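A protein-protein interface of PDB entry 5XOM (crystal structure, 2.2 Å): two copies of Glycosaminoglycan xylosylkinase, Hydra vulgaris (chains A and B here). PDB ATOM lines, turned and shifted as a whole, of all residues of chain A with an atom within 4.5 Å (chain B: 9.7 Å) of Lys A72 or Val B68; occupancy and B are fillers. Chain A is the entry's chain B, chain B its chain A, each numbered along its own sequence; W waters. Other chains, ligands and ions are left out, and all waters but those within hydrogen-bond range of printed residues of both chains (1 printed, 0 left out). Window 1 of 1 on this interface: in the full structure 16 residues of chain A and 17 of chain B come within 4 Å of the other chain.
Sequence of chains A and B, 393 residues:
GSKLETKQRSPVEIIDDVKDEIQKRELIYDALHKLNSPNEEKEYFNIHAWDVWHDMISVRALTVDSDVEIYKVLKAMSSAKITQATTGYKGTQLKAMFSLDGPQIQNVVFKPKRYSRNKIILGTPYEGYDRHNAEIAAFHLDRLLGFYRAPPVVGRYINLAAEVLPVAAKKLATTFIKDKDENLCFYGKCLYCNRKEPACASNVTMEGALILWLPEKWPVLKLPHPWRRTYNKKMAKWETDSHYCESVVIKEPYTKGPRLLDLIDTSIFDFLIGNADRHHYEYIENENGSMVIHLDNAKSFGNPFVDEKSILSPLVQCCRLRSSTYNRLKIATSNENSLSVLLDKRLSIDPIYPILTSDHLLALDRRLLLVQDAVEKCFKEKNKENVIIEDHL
Water W1 lies within hydrogen-bond range of the backbone NH of Asp B67 (3.0 Å), the side-chain carboxylate of Glu A69 (3.2 Å) and the backbone NH of Val B68 (3.3 Å).
Ile A47 touches Val B68, and with the chains exchanged Val A68 touches Ile B47. Ile A47 touches Tyr B71, and with the chains exchanged Tyr A71 touches Ile B47. Val A68 touches Glu B69, and with the chains exchanged Glu A69 touches Val B68. Val A68 touches Lys B72, and with the chains exchanged Lys A72 touches Val B68. Of the 17 pairs that touch across the chains among the printed residues, 10 have their exchanged pair printed and touching as well.
Of the 23 printed residues of chain B, 11 touch a printed residue of chain A. Printed residues of chain A that touch a printed residue of chain B: Ile A47, Val A52, Val A68, Glu A69, Tyr A71, Lys A72, Leu A74 and Lys A75. Hydrophobic or aromatic side chains of chain A that line the printed part of chain B: Ile A47, Val A52, Val A68, Tyr A71 and Leu A74. Among the printed residues, 17 pairs touch across the chains. Among the printed residues, no Asp or Glu carboxylate lies within 4 Å of a Lys or Arg side-chain nitrogen of the other chain.
The side-chain amino group (NZ) of Lys B72 sits close to the backbone carbonyl oxygen (O) of Ile B47. OG of Ser B66 sits close to N of Val B68 (3.4 Å). The side-chain hydroxyl of Ser B66 is in hydrogen-bond range of the backbone NH of Glu B69 (3.1 Å). The side-chain carboxylate (OD1) of Asp B67 lies within salt-bridge range of the guanidinium group (NH1) of Arg B143, at 3.5 Å. The backbone carbonyl oxygen (O) of Ile A47 lies within hydrogen-bond range of the side-chain amino group (NZ) of Lys A72 (3.1 Å).
Ile A47 touches three residues of chain B. Glu A69 touches just these residues of chain B: Ser B66 and Val B68. Of chain B, only Val B68 comes within 4 Å of Lys A72. No residue of chain B comes within 4 Å of Val A73. Of the printed residues of chain A, Val B52 touches Val A68. Of the printed residues of chain A, Asp B67 touches Ile A47 (3.8 Å). Printed residues of chain A within 4 Å of Val B68: Ile A47 (3.9 Å), Val A52 (3.6 Å), Glu A69 (3.7 Å) and Lys A72 (3.7 Å). Of the printed residues of chain A, Glu B69 touches Val A68. The nearest residue of chain B that does not touch Lys A72 is Phe B45 (5.3 Å). The nearest printed residue of chain A that does not touch Tyr B44 is Tyr A71 (5.9 Å).
NZ of Lys A75 lies within hydrogen-bond range of O of Tyr B44 (3.2 Å). OD1 of Asn B46 is in hydrogen-bond range of NZ of Lys A75 (3.4 Å). The side-chain hydroxyl of Ser B66 lies within hydrogen-bond range of the side-chain carboxylate of Glu A69 (2.8 Å).
Among the printed residues, pairs that only touch across the chains: Ile A47 with Asp B67, Ile A47 with Val B68, Ile A47 with Tyr B71, Val A52 with Val B68, Val A68 with Ile B47, Val A68 with Val B52, Val A68 with Glu B69, Val A68 with Lys B72, Glu A69 with Val B68, Tyr A71 with Phe B45, Tyr A71 with Ile B47, Lys A72 with Val B68, Leu A74 with Phe B45 and Lys A75 with Phe B45.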
ATOM      1  N   ILE A  47      -2.948  -0.164  13.669  1.00  0.00           N
ATOM      2  CA  ILE A  47      -3.170   1.085  12.950  1.00  0.00           C
ATOM      3  C   ILE A  47      -4.457   1.691  13.494  1.00  0.00           C
ATOM      4  O   ILE A  47      -5.481   1.005  13.577  1.00  0.00           O
ATOM      5  CB  ILE A  47      -3.275   0.877  11.425  1.00  0.00           C
ATOM      6  CG1 ILE A  47      -2.099   0.056  10.899  1.00  0.00           C
ATOM      7  CG2 ILE A  47      -3.343   2.215  10.705  1.00  0.00           C
ATOM      8  CD1 ILE A  47      -2.218  -0.276   9.434  1.00  0.00           C
ATOM      9  N   ALA A  49      -7.777   4.083  13.463  1.00  0.00           N
ATOM     10  CA  ALA A  49      -8.725   4.450  12.413  1.00  0.00           C
ATOM     11  C   ALA A  49      -8.518   5.879  11.923  1.00  0.00           C
ATOM     12  O   ALA A  49      -8.693   6.159  10.733  1.00  0.00           O
ATOM     13  CB  ALA A  49     -10.152   4.263  12.918  1.00  0.00           C
ATOM     14  N   VAL A  52      -5.926   5.781   9.405  1.00  0.00           N
ATOM     15  CA  VAL A  52      -6.461   5.205   8.176  1.00  0.00           C
ATOM     16  C   VAL A  52      -7.169   6.275   7.354  1.00  0.00           C
ATOM     17  O   VAL A  52      -6.971   6.379   6.137  1.00  0.00           O
ATOM     18  CB  VAL A  52      -7.398   4.028   8.508  1.00  0.00           C
ATOM     19  CG1 VAL A  52      -8.016   3.466   7.244  1.00  0.00           C
ATOM     20  CG2 VAL A  52      -6.647   2.949   9.261  1.00  0.00           C
ATOM     21  N   ASP A  67     -13.320  -2.319   1.635  1.00  0.00           N
ATOM     22  CA  ASP A  67     -14.298  -2.363   2.716  1.00  0.00           C
ATOM     23  C   ASP A  67     -13.627  -2.503   4.071  1.00  0.00           C
ATOM     24  O   ASP A  67     -14.159  -2.017   5.075  1.00  0.00           O
ATOM     25  CB  ASP A  67     -15.277  -3.517   2.512  1.00  0.00           C
ATOM     26  CG  ASP A  67     -16.280  -3.247   1.408  1.00  0.00           C
ATOM     27  OD1 ASP A  67     -16.362  -2.092   0.934  1.00  0.00           O
ATOM     28  OD2 ASP A  67     -16.995  -4.195   1.021  1.00  0.00           O
ATOM     29  N   VAL A  68     -12.475  -3.173   4.127  1.00  0.00           N
ATOM     30  CA  VAL A  68     -11.782  -3.327   5.401  1.00  0.00           C
ATOM     31  C   VAL A  68     -11.396  -1.962   5.950  1.00  0.00           C
ATOM     32  O   VAL A  68     -11.615  -1.666   7.129  1.00  0.00           O
ATOM     33  CB  VAL A  68     -10.557  -4.243   5.247  1.00  0.00           C
ATOM     34  CG1 VAL A  68      -9.784  -4.287   6.541  1.00  0.00           C
ATOM     35  CG2 VAL A  68     -10.992  -5.639   4.855  1.00  0.00           C
ATOM     36  N   GLU A  69     -10.838  -1.103   5.094  1.00  0.00           N
ATOM     37  CA  GLU A  69     -10.424   0.220   5.549  1.00  0.00           C
ATOM     38  C   GLU A  69     -11.623   1.090   5.912  1.00  0.00           C
ATOM     39  O   GLU A  69     -11.598   1.791   6.931  1.00  0.00           O
ATOM     40  CB  GLU A  69      -9.574   0.904   4.482  1.00  0.00           C
ATOM     41  CG  GLU A  69      -8.283   0.186   4.183  1.00  0.00           C
ATOM     42  CD  GLU A  69      -7.306   1.038   3.396  1.00  0.00           C
ATOM     43  OE1 GLU A  69      -7.487   2.272   3.349  1.00  0.00           O
ATOM     44  OE2 GLU A  69      -6.353   0.472   2.829  1.00  0.00           O
ATOM     45  N   ILE A  70     -12.681   1.062   5.096  1.00  0.00           N
ATOM     46  CA  ILE A  70     -13.827   1.931   5.358  1.00  0.00           C
ATOM     47  C   ILE A  70     -14.603   1.449   6.579  1.00  0.00           C
ATOM     48  O   ILE A  70     -14.957   2.250   7.453  1.00  0.00           O
ATOM     49  CB  ILE A  70     -14.720   2.036   4.107  1.00  0.00           C
ATOM     50  CG1 ILE A  70     -14.015   2.884   3.055  1.00  0.00           C
ATOM     51  CG2 ILE A  70     -16.037   2.696   4.441  1.00  0.00           C
ATOM     52  CD1 ILE A  70     -13.901   4.353   3.447  1.00  0.00           C
ATOM     53  N   TYR A  71     -14.856   0.136   6.679  1.00  0.00           N
ATOM     54  CA  TYR A  71     -15.549  -0.390   7.852  1.00  0.00           C
ATOM     55  C   TYR A  71     -14.757  -0.124   9.121  1.00  0.00           C
ATOM     56  O   TYR A  71     -15.344   0.096  10.188  1.00  0.00           O
ATOM     57  CB  TYR A  71     -15.802  -1.895   7.711  1.00  0.00           C
ATOM     58  CG  TYR A  71     -16.894  -2.299   6.738  1.00  0.00           C
ATOM     59  CD1 TYR A  71     -17.297  -1.453   5.712  1.00  0.00           C
ATOM     60  CD2 TYR A  71     -17.509  -3.545   6.835  1.00  0.00           C
ATOM     61  CE1 TYR A  71     -18.293  -1.831   4.817  1.00  0.00           C
ATOM     62  CE2 TYR A  71     -18.509  -3.931   5.942  1.00  0.00           C
ATOM     63  CZ  TYR A  71     -18.894  -3.069   4.939  1.00  0.00           C
ATOM     64  OH  TYR A  71     -19.880  -3.445   4.053  1.00  0.00           O
ATOM     65  N   LYS A  72     -13.429  -0.154   9.027  1.00  0.00           N
ATOM     66  CA  LYS A  72     -12.597   0.188  10.173  1.00  0.00           C
ATOM     67  C   LYS A  72     -12.848   1.624  10.616  1.00  0.00           C
ATOM     68  O   LYS A  72     -12.973   1.900  11.814  1.00  0.00           O
ATOM     69  CB  LYS A  72     -11.124  -0.027   9.819  1.00  0.00           C
ATOM     70  CG  LYS A  72     -10.138   0.211  10.949  1.00  0.00           C
ATOM     71  CD  LYS A  72      -8.731  -0.219  10.529  1.00  0.00           C
ATOM     72  CE  LYS A  72      -7.703   0.095  11.604  1.00  0.00           C
ATOM     73  NZ  LYS A  72      -7.744  -0.871  12.738  1.00  0.00           N
ATOM     74  N   VAL A  73     -12.956   2.547   9.659  1.00  0.00           N
ATOM     75  CA  VAL A  73     -13.191   3.946  10.004  1.00  0.00           C
ATOM     76  C   VAL A  73     -14.612   4.145  10.525  1.00  0.00           C
ATOM     77  O   VAL A  73     -14.821   4.790  11.558  1.00  0.00           O
ATOM     78  CB  VAL A  73     -12.881   4.844   8.793  1.00  0.00           C
ATOM     79  CG1 VAL A  73     -13.282   6.283   9.072  1.00  0.00           C
ATOM     80  CG2 VAL A  73     -11.400   4.768   8.469  1.00  0.00           C
ATOM     81  N   LEU A  74     -15.606   3.566   9.841  1.00  0.00           N
ATOM     82  CA  LEU A  74     -16.998   3.720  10.272  1.00  0.00           C
ATOM     83  C   LEU A  74     -17.212   3.159  11.674  1.00  0.00           C
ATOM     84  O   LEU A  74     -17.910   3.766  12.498  1.00  0.00           O
ATOM     85  CB  LEU A  74     -17.936   3.028   9.277  1.00  0.00           C
ATOM     86  CG  LEU A  74     -17.904   3.538   7.831  1.00  0.00           C
ATOM     87  CD1 LEU A  74     -18.976   2.872   6.969  1.00  0.00           C
ATOM     88  CD2 LEU A  74     -18.042   5.065   7.801  1.00  0.00           C
ATOM     89  N   LYS A  75     -16.625   1.993  11.958  1.00  0.00           N
ATOM     90  CA  LYS A  75     -16.767   1.386  13.279  1.00  0.00           C
ATOM     91  C   LYS A  75     -16.207   2.296  14.362  1.00  0.00           C
ATOM     92  O   LYS A  75     -16.793   2.421  15.442  1.00  0.00           O
ATOM     93  CB  LYS A  75     -16.073   0.024  13.304  1.00  0.00           C
ATOM     94  CG  LYS A  75     -16.238  -0.749  14.608  1.00  0.00           C
ATOM     95  CD  LYS A  75     -15.566  -2.115  14.511  1.00  0.00           C
ATOM     96  CE  LYS A  75     -15.688  -2.905  15.807  1.00  0.00           C
ATOM     97  NZ  LYS A  75     -17.107  -3.179  16.172  1.00  0.00           N
ATOM     98  N   ALA A  76     -15.075   2.944  14.092  1.00  0.00           N
ATOM     99  CA  ALA A  76     -14.515   3.860  15.078  1.00  0.00           C
ATOM    100  C   ALA A  76     -15.397   5.090  15.260  1.00  0.00           C
ATOM    101  O   ALA A  76     -15.606   5.539  16.392  1.00  0.00           O
ATOM    102  CB  ALA A  76     -13.103   4.271  14.673  1.00  0.00           C
ATOM    103  N   TYR B  44     -21.262  -3.905  14.918  1.00  0.00           N
ATOM    104  CA  TYR B  44     -21.316  -3.398  13.556  1.00  0.00           C
ATOM    105  C   TYR B  44     -19.938  -3.379  12.902  1.00  0.00           C
ATOM    106  O   TYR B  44     -18.916  -3.197  13.571  1.00  0.00           O
ATOM    107  CB  TYR B  44     -21.907  -1.978  13.555  1.00  0.00           C
ATOM    108  CG  TYR B  44     -23.335  -1.930  14.048  1.00  0.00           C
ATOM    109  CD1 TYR B  44     -24.379  -2.381  13.252  1.00  0.00           C
ATOM    110  CD2 TYR B  44     -23.635  -1.459  15.324  1.00  0.00           C
ATOM    111  CE1 TYR B  44     -25.684  -2.351  13.701  1.00  0.00           C
ATOM    112  CE2 TYR B  44     -24.938  -1.425  15.786  1.00  0.00           C
ATOM    113  CZ  TYR B  44     -25.960  -1.874  14.968  1.00  0.00           C
ATOM    114  OH  TYR B  44     -27.264  -1.851  15.406  1.00  0.00           O
ATOM    115  N   PHE B  45     -19.933  -3.587  11.580  1.00  0.00           N
ATOM    116  CA  PHE B  45     -18.766  -3.394  10.715  1.00  0.00           C
ATOM    117  C   PHE B  45     -17.646  -4.407  10.963  1.00  0.00           C
ATOM    118  O   PHE B  45     -16.470  -4.078  10.803  1.00  0.00           O
ATOM    119  CB  PHE B  45     -18.208  -1.973  10.859  1.00  0.00           C
ATOM    120  CG  PHE B  45     -19.218  -0.890  10.600  1.00  0.00           C
ATOM    121  CD1 PHE B  45     -19.622  -0.587   9.312  1.00  0.00           C
ATOM    122  CD2 PHE B  45     -19.748  -0.158  11.651  1.00  0.00           C
ATOM    123  CE1 PHE B  45     -20.553   0.414   9.081  1.00  0.00           C
ATOM    124  CE2 PHE B  45     -20.673   0.840  11.428  1.00  0.00           C
ATOM    125  CZ  PHE B  45     -21.077   1.128  10.140  1.00  0.00           C
ATOM    126  N   ASN B  46     -17.972  -5.645  11.322  1.00  0.00           N
ATOM    127  CA  ASN B  46     -16.953  -6.635  11.652  1.00  0.00           C
ATOM    128  C   ASN B  46     -16.561  -7.454  10.425  1.00  0.00           C
ATOM    129  O   ASN B  46     -17.424  -7.999   9.732  1.00  0.00           O
ATOM    130  CB  ASN B  46     -17.455  -7.552  12.765  1.00  0.00           C
ATOM    131  CG  ASN B  46     -17.424  -6.881  14.126  1.00  0.00           C
ATOM    132  OD1 ASN B  46     -16.610  -5.992  14.376  1.00  0.00           O
ATOM    133  ND2 ASN B  46     -18.322  -7.298  15.009  1.00  0.00           N
ATOM    134  N   ILE B  47     -15.255  -7.559  10.179  1.00  0.00           N
ATOM    135  CA  ILE B  47     -14.688  -8.458   9.175  1.00  0.00           C
ATOM    136  C   ILE B  47     -13.588  -9.270   9.844  1.00  0.00           C
ATOM    137  O   ILE B  47     -12.706  -8.699  10.496  1.00  0.00           O
ATOM    138  CB  ILE B  47     -14.123  -7.686   7.968  1.00  0.00           C
ATOM    139  CG1 ILE B  47     -15.159  -6.687   7.438  1.00  0.00           C
ATOM    140  CG2 ILE B  47     -13.666  -8.658   6.874  1.00  0.00           C
ATOM    141  CD1 ILE B  47     -14.642  -5.791   6.331  1.00  0.00           C
ATOM    142  N   ALA B  49     -10.206 -11.561  10.060  1.00  0.00           N
ATOM    143  CA  ALA B  49      -8.939 -11.533   9.336  1.00  0.00           C
ATOM    144  C   ALA B  49      -8.808 -12.689   8.348  1.00  0.00           C
ATOM    145  O   ALA B  49      -8.255 -12.512   7.257  1.00  0.00           O
ATOM    146  CB  ALA B  49      -7.778 -11.544  10.325  1.00  0.00           C
ATOM    147  N   VAL B  52     -10.378 -11.685   5.235  1.00  0.00           N
ATOM    148  CA  VAL B  52      -9.536 -10.718   4.536  1.00  0.00           C
ATOM    149  C   VAL B  52      -8.463 -11.434   3.725  1.00  0.00           C
ATOM    150  O   VAL B  52      -8.179 -11.064   2.580  1.00  0.00           O
ATOM    151  CB  VAL B  52      -8.920  -9.722   5.535  1.00  0.00           C
ATOM    152  CG1 VAL B  52      -7.969  -8.772   4.819  1.00  0.00           C
ATOM    153  CG2 VAL B  52     -10.025  -8.949   6.257  1.00  0.00           C
ATOM    154  N   TRP B  53      -7.850 -12.467   4.312  1.00  0.00           N
ATOM    155  CA  TRP B  53      -6.836 -13.251   3.611  1.00  0.00           C
ATOM    156  C   TRP B  53      -7.433 -13.976   2.410  1.00  0.00           C
ATOM    157  O   TRP B  53      -6.882 -13.927   1.304  1.00  0.00           O
ATOM    158  CB  TRP B  53      -6.192 -14.241   4.588  1.00  0.00           C
ATOM    159  CG  TRP B  53      -5.312 -15.327   3.992  1.00  0.00           C
ATOM    160  CD1 TRP B  53      -5.343 -16.659   4.299  1.00  0.00           C
ATOM    161  CD2 TRP B  53      -4.265 -15.169   3.020  1.00  0.00           C
ATOM    162  NE1 TRP B  53      -4.391 -17.341   3.579  1.00  0.00           N
ATOM    163  CE2 TRP B  53      -3.715 -16.450   2.786  1.00  0.00           C
ATOM    164  CE3 TRP B  53      -3.742 -14.073   2.323  1.00  0.00           C
ATOM    165  CZ2 TRP B  53      -2.666 -16.663   1.890  1.00  0.00           C
ATOM    166  CZ3 TRP B  53      -2.702 -14.287   1.426  1.00  0.00           C
ATOM    167  CH2 TRP B  53      -2.176 -15.575   1.218  1.00  0.00           C
ATOM    168  N   MET B  56      -8.355 -11.450  -0.553  1.00  0.00           N
ATOM    169  CA  MET B  56      -7.396 -10.561  -1.193  1.00  0.00           C
ATOM    170  C   MET B  56      -6.620 -11.234  -2.319  1.00  0.00           C
ATOM    171  O   MET B  56      -6.010 -10.531  -3.131  1.00  0.00           O
ATOM    172  CB  MET B  56      -6.413  -9.973  -0.159  1.00  0.00           C
ATOM    173  CG  MET B  56      -5.272 -10.886   0.277  1.00  0.00           C
ATOM    174  SD  MET B  56      -3.990 -10.029   1.247  1.00  0.00           S
ATOM    175  CE  MET B  56      -4.936  -9.367   2.619  1.00  0.00           C
ATOM    176  N   VAL B  64      -1.771  -7.349  -1.161  1.00  0.00           N
ATOM    177  CA  VAL B  64      -2.159  -6.059  -1.711  1.00  0.00           C
ATOM    178  C   VAL B  64      -1.346  -4.956  -1.046  1.00  0.00           C
ATOM    179  O   VAL B  64      -0.698  -5.155  -0.018  1.00  0.00           O
ATOM    180  CB  VAL B  64      -3.665  -5.791  -1.536  1.00  0.00           C
ATOM    181  CG1 VAL B  64      -4.465  -6.746  -2.395  1.00  0.00           C
ATOM    182  CG2 VAL B  64      -4.049  -5.930  -0.068  1.00  0.00           C
ATOM    183  N   ASP B  65      -1.412  -3.770  -1.653  1.00  0.00           N
ATOM    184  CA  ASP B  65      -0.675  -2.609  -1.171  1.00  0.00           C
ATOM    185  C   ASP B  65      -1.190  -2.110   0.175  1.00  0.00           C
ATOM    186  O   ASP B  65      -0.437  -1.460   0.909  1.00  0.00           O
ATOM    187  CB  ASP B  65      -0.746  -1.499  -2.222  1.00  0.00           C
ATOM    188  CG  ASP B  65      -0.006  -0.243  -1.805  1.00  0.00           C
ATOM    189  OD1 ASP B  65       1.101  -0.362  -1.239  1.00  0.00           O
ATOM    190  OD2 ASP B  65      -0.525   0.864  -2.057  1.00  0.00           O
ATOM    191  N   SER B  66      -2.444  -2.407   0.516  1.00  0.00           N
ATOM    192  CA  SER B  66      -3.092  -1.873   1.715  1.00  0.00           C
ATOM    193  C   SER B  66      -2.436  -2.402   2.987  1.00  0.00           C
ATOM    194  O   SER B  66      -2.576  -3.582   3.324  1.00  0.00           O
ATOM    195  CB  SER B  66      -4.574  -2.233   1.701  1.00  0.00           C
ATOM    196  OG  SER B  66      -5.153  -2.004   2.975  1.00  0.00           O
ATOM    197  N   ASP B  67      -1.786  -1.508   3.736  1.00  0.00           N
ATOM    198  CA  ASP B  67      -1.228  -1.889   5.028  1.00  0.00           C
ATOM    199  C   ASP B  67      -2.320  -2.229   6.030  1.00  0.00           C
ATOM    200  O   ASP B  67      -2.108  -3.065   6.916  1.00  0.00           O
ATOM    201  CB  ASP B  67      -0.342  -0.771   5.578  1.00  0.00           C
ATOM    202  CG  ASP B  67       0.979  -0.654   4.836  1.00  0.00           C
ATOM    203  OD1 ASP B  67       1.303  -1.566   4.042  1.00  0.00           O
ATOM    204  OD2 ASP B  67       1.696   0.348   5.053  1.00  0.00           O
ATOM    205  N   VAL B  68      -3.488  -1.592   5.917  1.00  0.00           N
ATOM    206  CA  VAL B  68      -4.580  -1.880   6.841  1.00  0.00           C
ATOM    207  C   VAL B  68      -5.015  -3.332   6.709  1.00  0.00           C
ATOM    208  O   VAL B  68      -5.181  -4.045   7.706  1.00  0.00           O
ATOM    209  CB  VAL B  68      -5.754  -0.911   6.612  1.00  0.00           C
ATOM    210  CG1 VAL B  68      -6.924  -1.292   7.492  1.00  0.00           C
ATOM    211  CG2 VAL B  68      -5.315   0.512   6.906  1.00  0.00           C
ATOM    212  N   GLU B  69      -5.193  -3.794   5.472  1.00  0.00           N
ATOM    213  CA  GLU B  69      -5.629  -5.171   5.254  1.00  0.00           C
ATOM    214  C   GLU B  69      -4.553  -6.168   5.678  1.00  0.00           C
ATOM    215  O   GLU B  69      -4.861  -7.189   6.305  1.00  0.00           O
ATOM    216  CB  GLU B  69      -6.014  -5.371   3.789  1.00  0.00           C
ATOM    217  CG  GLU B  69      -7.200  -4.518   3.346  1.00  0.00           C
ATOM    218  CD  GLU B  69      -7.777  -4.947   2.003  1.00  0.00           C
ATOM    219  OE1 GLU B  69      -7.473  -6.070   1.553  1.00  0.00           O
ATOM    220  OE2 GLU B  69      -8.548  -4.168   1.403  1.00  0.00           O
ATOM    221  N   ILE B  70      -3.288  -5.885   5.357  1.00  0.00           N
ATOM    222  CA  ILE B  70      -2.209  -6.823   5.667  1.00  0.00           C
ATOM    223  C   ILE B  70      -1.928  -6.855   7.167  1.00  0.00           C
ATOM    224  O   ILE B  70      -1.798  -7.935   7.760  1.00  0.00           O
ATOM    225  CB  ILE B  70      -0.950  -6.483   4.849  1.00  0.00           C
ATOM    226  CG1 ILE B  70      -1.178  -6.872   3.390  1.00  0.00           C
ATOM    227  CG2 ILE B  70       0.257  -7.231   5.374  1.00  0.00           C
ATOM    228  CD1 ILE B  70      -1.263  -8.384   3.191  1.00  0.00           C
ATOM    229  N   TYR B  71      -1.844  -5.682   7.813  1.00  0.00           N
ATOM    230  CA  TYR B  71      -1.620  -5.670   9.262  1.00  0.00           C
ATOM    231  C   TYR B  71      -2.751  -6.358  10.008  1.00  0.00           C
ATOM    232  O   TYR B  71      -2.521  -6.972  11.055  1.00  0.00           O
ATOM    233  CB  TYR B  71      -1.460  -4.246   9.803  1.00  0.00           C
ATOM    234  CG  TYR B  71      -0.151  -3.572   9.460  1.00  0.00           C
ATOM    235  CD1 TYR B  71       0.584  -3.960   8.346  1.00  0.00           C
ATOM    236  CD2 TYR B  71       0.369  -2.568  10.273  1.00  0.00           C
ATOM    237  CE1 TYR B  71       1.775  -3.346   8.026  1.00  0.00           C
ATOM    238  CE2 TYR B  71       1.572  -1.947   9.962  1.00  0.00           C
ATOM    239  CZ  TYR B  71       2.264  -2.343   8.835  1.00  0.00           C
ATOM    240  OH  TYR B  71       3.459  -1.751   8.501  1.00  0.00           O
ATOM    241  N   LYS B  72      -3.978  -6.261   9.496  1.00  0.00           N
ATOM    242  CA  LYS B  72      -5.091  -6.967  10.118  1.00  0.00           C
ATOM    243  C   LYS B  72      -4.844  -8.470  10.125  1.00  0.00           C
ATOM    244  O   LYS B  72      -5.127  -9.153  11.117  1.00  0.00           O
ATOM    245  CB  LYS B  72      -6.385  -6.628   9.378  1.00  0.00           C
ATOM    246  CG  LYS B  72      -7.654  -7.208   9.977  1.00  0.00           C
ATOM    247  CD  LYS B  72      -8.858  -6.637   9.243  1.00  0.00           C
ATOM    248  CE  LYS B  72     -10.146  -7.209   9.763  1.00  0.00           C
ATOM    249  NZ  LYS B  72     -10.535  -6.549  11.037  1.00  0.00           N
ATOM    250  N   VAL B  73      -4.323  -9.003   9.016  1.00  0.00           N
ATOM    251  CA  VAL B  73      -4.032 -10.430   8.937  1.00  0.00           C
ATOM    252  C   VAL B  73      -2.828 -10.781   9.809  1.00  0.00           C
ATOM    253  O   VAL B  73      -2.858 -11.760  10.563  1.00  0.00           O
ATOM    254  CB  VAL B  73      -3.827 -10.842   7.467  1.00  0.00           C
ATOM    255  CG1 VAL B  73      -3.362 -12.293   7.372  1.00  0.00           C
ATOM    256  CG2 VAL B  73      -5.119 -10.641   6.681  1.00  0.00           C
ATOM    257  N   LEU B  74      -1.760  -9.977   9.739  1.00  0.00           N
ATOM    258  CA  LEU B  74      -0.566 -10.239  10.546  1.00  0.00           C
ATOM    259  C   LEU B  74      -0.882 -10.200  12.037  1.00  0.00           C
ATOM    260  O   LEU B  74      -0.392 -11.035  12.809  1.00  0.00           O
ATOM    261  CB  LEU B  74       0.533  -9.229  10.208  1.00  0.00           C
ATOM    262  CG  LEU B  74       1.055  -9.226   8.769  1.00  0.00           C
ATOM    263  CD1 LEU B  74       2.199  -8.212   8.610  1.00  0.00           C
ATOM    264  CD2 LEU B  74       1.532 -10.631   8.377  1.00  0.00           C
ATOM    265  N   LYS B  75      -1.696  -9.233  12.465  1.00  0.00           N
ATOM    266  CA  LYS B  75      -2.070  -9.155  13.875  1.00  0.00           C
ATOM    267  C   LYS B  75      -2.805 -10.413  14.320  1.00  0.00           C
ATOM    268  O   LYS B  75      -2.574 -10.920  15.425  1.00  0.00           O
ATOM    269  CB  LYS B  75      -2.938  -7.920  14.117  1.00  0.00           C
ATOM    270  CG  LYS B  75      -3.330  -7.690  15.573  1.00  0.00           C
ATOM    271  CD  LYS B  75      -4.175  -6.427  15.690  1.00  0.00           C
ATOM    272  CE  LYS B  75      -4.616  -6.177  17.117  1.00  0.00           C
ATOM    273  NZ  LYS B  75      -3.434  -5.986  17.992  1.00  0.00           N
ATOM    274  N   ALA B  76      -3.688 -10.939  13.473  1.00  0.00           N
ATOM    275  CA  ALA B  76      -4.405 -12.156  13.840  1.00  0.00           C
ATOM    276  C   ALA B  76      -3.462 -13.349  13.922  1.00  0.00           C
ATOM    277  O   ALA B  76      -3.582 -14.177  14.831  1.00  0.00           O
ATOM    278  CB  ALA B  76      -5.528 -12.430  12.842  1.00  0.00           C
ATOM    279  N   ARG B 143       6.611  -7.393  -0.714  1.00  0.00           N
ATOM    280  CA  ARG B 143       5.677  -6.272  -0.800  1.00  0.00           C
ATOM    281  C   ARG B 143       6.399  -4.979  -1.163  1.00  0.00           C
ATOM    282  O   ARG B 143       5.908  -4.200  -1.989  1.00  0.00           O
ATOM    283  CB  ARG B 143       4.927  -6.119   0.521  1.00  0.00           C
ATOM    284  CG  ARG B 143       4.230  -7.388   0.951  1.00  0.00           C
ATOM    285  CD  ARG B 143       3.330  -7.159   2.141  1.00  0.00           C
ATOM    286  NE  ARG B 143       2.184  -6.327   1.782  1.00  0.00           N
ATOM    287  CZ  ARG B 143       1.946  -5.128   2.298  1.00  0.00           C
ATOM    288  NH1 ARG B 143       2.768  -4.620   3.210  1.00  0.00           N
ATOM    289  NH2 ARG B 143       0.883  -4.436   1.916  1.00  0.00           N
ATOM    290  N   ILE B 349       8.078  -3.521  12.687  1.00  0.00           N
ATOM    291  CA  ILE B 349       6.777  -3.801  13.290  1.00  0.00           C
ATOM    292  C   ILE B 349       6.642  -5.248  13.741  1.00  0.00           C
ATOM    293  O   ILE B 349       5.709  -5.567  14.496  1.00  0.00           O
ATOM    294  CB  ILE B 349       5.624  -3.480  12.312  1.00  0.00           C
ATOM    295  CG1 ILE B 349       5.505  -4.592  11.271  1.00  0.00           C
ATOM    296  CG2 ILE B 349       5.854  -2.130  11.610  1.00  0.00           C
ATOM    297  CD1 ILE B 349       4.546  -4.301  10.161  1.00  0.00           C
HETATM  298  O   HOH W   1      -3.403   1.031   3.922  1.00  0.00           O
